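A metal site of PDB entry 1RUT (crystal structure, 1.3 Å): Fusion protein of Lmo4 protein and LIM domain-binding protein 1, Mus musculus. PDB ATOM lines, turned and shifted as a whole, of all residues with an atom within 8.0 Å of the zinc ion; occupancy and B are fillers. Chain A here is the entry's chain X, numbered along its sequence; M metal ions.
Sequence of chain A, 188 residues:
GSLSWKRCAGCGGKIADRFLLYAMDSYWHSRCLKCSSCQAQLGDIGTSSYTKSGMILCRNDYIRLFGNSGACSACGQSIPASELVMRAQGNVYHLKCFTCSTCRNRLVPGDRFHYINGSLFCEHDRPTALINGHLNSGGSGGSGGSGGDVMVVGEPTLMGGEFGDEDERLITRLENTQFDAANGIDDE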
ATOM      1  N   ALA A  71      19.338 -32.071 -17.866  1.00  0.00           N
ATOM      2  CA  ALA A  71      18.775 -32.727 -16.698  1.00  0.00           C
ATOM      3  C   ALA A  71      18.661 -31.713 -15.592  1.00  0.00           C
ATOM      4  O   ALA A  71      19.505 -30.821 -15.465  1.00  0.00           O
ATOM      5  CB  ALA A  71      19.643 -33.900 -16.270  1.00  0.00           C
ATOM      6  N   CYS A  72      17.606 -31.846 -14.808  1.00  0.00           N
ATOM      7  CA  CYS A  72      17.293 -30.918 -13.725  1.00  0.00           C
ATOM      8  C   CYS A  72      18.172 -31.213 -12.517  1.00  0.00           C
ATOM      9  O   CYS A  72      18.197 -32.330 -12.025  1.00  0.00           O
ATOM     10  CB  CYS A  72      15.835 -31.081 -13.333  1.00  0.00           C
ATOM     11  SG  CYS A  72      15.278 -29.971 -12.043  1.00  0.00           S
ATOM     12  N   SER A  73      18.887 -30.199 -12.038  1.00  0.00           N
ATOM     13  CA  SER A  73      19.746 -30.392 -10.874  1.00  0.00           C
ATOM     14  C   SER A  73      18.968 -30.638  -9.580  1.00  0.00           C
ATOM     15  O   SER A  73      19.537 -31.157  -8.616  1.00  0.00           O
ATOM     16  CB  SER A  73      20.674 -29.194 -10.688  1.00  0.00           C
ATOM     17  OG  SER A  73      21.760 -29.262 -11.604  1.00  0.00           O
ATOM     18  N   ALA A  74      17.696 -30.247  -9.549  1.00  0.00           N
ATOM     19  CA  ALA A  74      16.872 -30.455  -8.362  1.00  0.00           C
ATOM     20  C   ALA A  74      16.335 -31.881  -8.307  1.00  0.00           C
ATOM     21  O   ALA A  74      16.582 -32.576  -7.327  1.00  0.00           O
ATOM     22  CB  ALA A  74      15.730 -29.458  -8.314  1.00  0.00           C
ATOM     23  N   CYS A  75      15.623 -32.316  -9.336  1.00  0.00           N
ATOM     24  CA  CYS A  75      14.948 -33.617  -9.303  1.00  0.00           C
ATOM     25  C   CYS A  75      15.669 -34.740 -10.052  1.00  0.00           C
ATOM     26  O   CYS A  75      15.259 -35.890  -9.958  1.00  0.00           O
ATOM     27  CB  CYS A  75      13.521 -33.496  -9.839  1.00  0.00           C
ATOM     28  SG  CYS A  75      13.414 -33.254 -11.621  1.00  0.00           S
ATOM     29  N   GLY A  76      16.724 -34.396 -10.785  1.00  0.00           N
ATOM     30  CA  GLY A  76      17.544 -35.357 -11.504  1.00  0.00           C
ATOM     31  C   GLY A  76      17.003 -35.827 -12.840  1.00  0.00           C
ATOM     32  O   GLY A  76      17.702 -36.546 -13.571  1.00  0.00           O
ATOM     33  N   GLN A  77      15.777 -35.457 -13.165  1.00  0.00           N
ATOM     34  CA  GLN A  77      15.104 -36.002 -14.339  1.00  0.00           C
ATOM     35  C   GLN A  77      15.465 -35.238 -15.619  1.00  0.00           C
ATOM     36  O   GLN A  77      15.788 -34.056 -15.583  1.00  0.00           O
ATOM     37  CB  GLN A  77      13.586 -35.998 -14.146  1.00  0.00           C
ATOM     38  CG  GLN A  77      13.096 -36.732 -12.907  1.00  0.00           C
ATOM     39  CD  GLN A  77      11.583 -36.817 -12.829  1.00  0.00           C
ATOM     40  OE1 GLN A  77      10.993 -37.817 -13.236  1.00  0.00           O
ATOM     41  NE2 GLN A  77      10.957 -35.778 -12.301  1.00  0.00           N
ATOM     42  N   SER A  78      15.388 -35.936 -16.745  1.00  0.00           N
ATOM     43  CA  SER A  78      15.733 -35.344 -18.033  1.00  0.00           C
ATOM     44  C   SER A  78      14.847 -34.142 -18.383  1.00  0.00           C
ATOM     45  O   SER A  78      13.688 -34.047 -17.973  1.00  0.00           O
ATOM     46  CB  SER A  78      15.639 -36.411 -19.138  1.00  0.00           C
ATOM     47  OG  SER A  78      14.338 -36.980 -19.177  1.00  0.00           O
ATOM     48  N   ILE A  79      15.423 -33.205 -19.133  1.00  0.00           N
ATOM     49  CA  ILE A  79      14.714 -32.043 -19.654  1.00  0.00           C
ATOM     50  C   ILE A  79      14.907 -32.057 -21.165  1.00  0.00           C
ATOM     51  O   ILE A  79      16.036 -31.976 -21.636  1.00  0.00           O
ATOM     52  CB  ILE A  79      15.280 -30.730 -19.093  1.00  0.00           C
ATOM     53  CG1 ILE A  79      15.244 -30.727 -17.560  1.00  0.00           C
ATOM     54  CG2 ILE A  79      14.497 -29.532 -19.644  1.00  0.00           C
ATOM     55  CD1 ILE A  79      15.979 -29.549 -16.947  1.00  0.00           C
ATOM     56  N   GLU A  83      12.269 -27.646 -23.947  1.00  0.00           N
ATOM     57  CA  GLU A  83      11.634 -27.134 -22.737  1.00  0.00           C
ATOM     58  C   GLU A  83      12.363 -25.900 -22.199  1.00  0.00           C
ATOM     59  O   GLU A  83      13.580 -25.860 -22.194  1.00  0.00           O
ATOM     60  CB  GLU A  83      11.560 -28.236 -21.673  1.00  0.00           C
ATOM     61  CG  GLU A  83      10.795 -27.836 -20.427  1.00  0.00           C
ATOM     62  CD  GLU A  83      10.518 -28.987 -19.489  1.00  0.00           C
ATOM     63  OE1 GLU A  83      10.445 -30.139 -19.931  1.00  0.00           O
ATOM     64  OE2 GLU A  83      10.360 -28.723 -18.274  1.00  0.00           O
ATOM     65  N   VAL A  92      20.777 -26.290 -14.533  1.00  0.00           N
ATOM     66  CA  VAL A  92      19.469 -26.026 -15.121  1.00  0.00           C
ATOM     67  C   VAL A  92      18.376 -26.723 -14.295  1.00  0.00           C
ATOM     68  O   VAL A  92      18.611 -27.743 -13.659  1.00  0.00           O
ATOM     69  CB  VAL A  92      19.395 -26.398 -16.620  1.00  0.00           C
ATOM     70  CG1 VAL A  92      20.350 -25.519 -17.420  1.00  0.00           C
ATOM     71  CG2 VAL A  92      19.704 -27.867 -16.840  1.00  0.00           C
ATOM     72  N   TYR A  93      17.188 -26.134 -14.315  1.00  0.00           N
ATOM     73  CA  TYR A  93      16.058 -26.594 -13.501  1.00  0.00           C
ATOM     74  C   TYR A  93      14.760 -26.546 -14.297  1.00  0.00           C
ATOM     75  O   TYR A  93      14.534 -25.606 -15.050  1.00  0.00           O
ATOM     76  CB  TYR A  93      15.878 -25.701 -12.283  1.00  0.00           C
ATOM     77  CG  TYR A  93      17.076 -25.653 -11.382  1.00  0.00           C
ATOM     78  CD1 TYR A  93      18.099 -24.734 -11.598  1.00  0.00           C
ATOM     79  CD2 TYR A  93      17.203 -26.534 -10.308  1.00  0.00           C
ATOM     80  CE1 TYR A  93      19.216 -24.695 -10.777  1.00  0.00           C
ATOM     81  CE2 TYR A  93      18.307 -26.501  -9.484  1.00  0.00           C
ATOM     82  CZ  TYR A  93      19.312 -25.571  -9.721  1.00  0.00           C
ATOM     83  OH  TYR A  93      20.419 -25.524  -8.921  1.00  0.00           O
ATOM     84  N   HIS A  94      13.899 -27.545 -14.104  1.00  0.00           N
ATOM     85  CA  HIS A  94      12.481 -27.401 -14.439  1.00  0.00           C
ATOM     86  C   HIS A  94      11.969 -26.145 -13.753  1.00  0.00           C
ATOM     87  O   HIS A  94      12.343 -25.855 -12.620  1.00  0.00           O
ATOM     88  CB  HIS A  94      11.644 -28.571 -13.948  1.00  0.00           C
ATOM     89  CG  HIS A  94      11.958 -29.886 -14.602  1.00  0.00           C
ATOM     90  ND1 HIS A  94      12.535 -30.934 -13.913  1.00  0.00           N
ATOM     91  CD2 HIS A  94      11.736 -30.334 -15.853  1.00  0.00           C
ATOM     92  CE1 HIS A  94      12.671 -31.967 -14.726  1.00  0.00           C
ATOM     93  NE2 HIS A  94      12.200 -31.620 -15.911  1.00  0.00           N
ATOM     94  N   LEU A  95      11.076 -25.415 -14.422  1.00  0.00           N
ATOM     95  CA  LEU A  95      10.497 -24.222 -13.804  1.00  0.00           C
ATOM     96  C   LEU A  95       9.895 -24.524 -12.438  1.00  0.00           C
ATOM     97  O   LEU A  95      10.108 -23.767 -11.481  1.00  0.00           O
ATOM     98  CB  LEU A  95       9.440 -23.562 -14.703  1.00  0.00           C
ATOM     99  CG  LEU A  95       9.975 -22.441 -15.577  1.00  0.00           C
ATOM    100  CD1 LEU A  95      11.057 -22.932 -16.491  1.00  0.00           C
ATOM    101  CD2 LEU A  95       8.854 -21.801 -16.389  1.00  0.00           C
ATOM    102  N   LYS A  96       9.162 -25.630 -12.321  1.00  0.00           N
ATOM    103  CA  LYS A  96       8.467 -25.938 -11.075  1.00  0.00           C
ATOM    104  C   LYS A  96       9.390 -26.551 -10.013  1.00  0.00           C
ATOM    105  O   LYS A  96       8.991 -26.684  -8.853  1.00  0.00           O
ATOM    106  CB  LYS A  96       7.244 -26.831 -11.357  1.00  0.00           C
ATOM    107  CG  LYS A  96       6.140 -26.086 -12.093  1.00  0.00           C
ATOM    108  CD  LYS A  96       4.881 -26.916 -12.271  1.00  0.00           C
ATOM    109  CE  LYS A  96       3.818 -26.169 -13.066  1.00  0.00           C
ATOM    110  NZ  LYS A  96       2.564 -26.958 -13.213  1.00  0.00           N
ATOM    111  N   CYS A  97      10.614 -26.898 -10.391  1.00  0.00           N
ATOM    112  CA  CYS A  97      11.647 -27.352  -9.446  1.00  0.00           C
ATOM    113  C   CYS A  97      12.522 -26.213  -8.927  1.00  0.00           C
ATOM    114  O   CYS A  97      13.336 -26.401  -8.017  1.00  0.00           O
ATOM    115  CB  CYS A  97      12.553 -28.380 -10.119  1.00  0.00           C
ATOM    116  SG  CYS A  97      11.756 -29.948 -10.460  1.00  0.00           S
ATOM    117  N   PHE A  98      12.366 -25.035  -9.498  1.00  0.00           N
ATOM    118  CA  PHE A  98      13.193 -23.881  -9.163  1.00  0.00           C
ATOM    119  C   PHE A  98      12.520 -23.156  -8.011  1.00  0.00           C
ATOM    120  O   PHE A  98      11.872 -22.123  -8.197  1.00  0.00           O
ATOM    121  CB  PHE A  98      13.365 -22.993 -10.406  1.00  0.00           C
ATOM    122  CG  PHE A  98      14.498 -22.019 -10.319  1.00  0.00           C
ATOM    123  CD1 PHE A  98      15.816 -22.443 -10.264  1.00  0.00           C
ATOM    124  CD2 PHE A  98      14.246 -20.659 -10.298  1.00  0.00           C
ATOM    125  CE1 PHE A  98      16.854 -21.531 -10.190  1.00  0.00           C
ATOM    126  CE2 PHE A  98      15.273 -19.746 -10.233  1.00  0.00           C
ATOM    127  CZ  PHE A  98      16.579 -20.176 -10.175  1.00  0.00           C
HETATM  128 ZN    ZN M   1      13.174 -30.983 -11.901  1.00  0.00          ZN
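SG of Cys 75 sits close to N of Gln 77 (3.6 Å). N of Ala 74 sits close to SG of Cys 72. The backbone carbonyl oxygen of Gln 77 is in hydrogen-bond range of the backbone NH of Cys 72 (3.0 Å).
The nearest printed residue that does not touch the zinc ion is Ala 74 (4.7 Å).
ND1 of His 94 is bound to the zinc ion, 2.1 Å away. SG of Cys 97 binds the zinc ion (2.3 Å). The zinc ion is bound by SG of Cys 75, 2.3 Å away. The zinc ion is bound by the side-chain sulfur (SG) of Cys 72.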
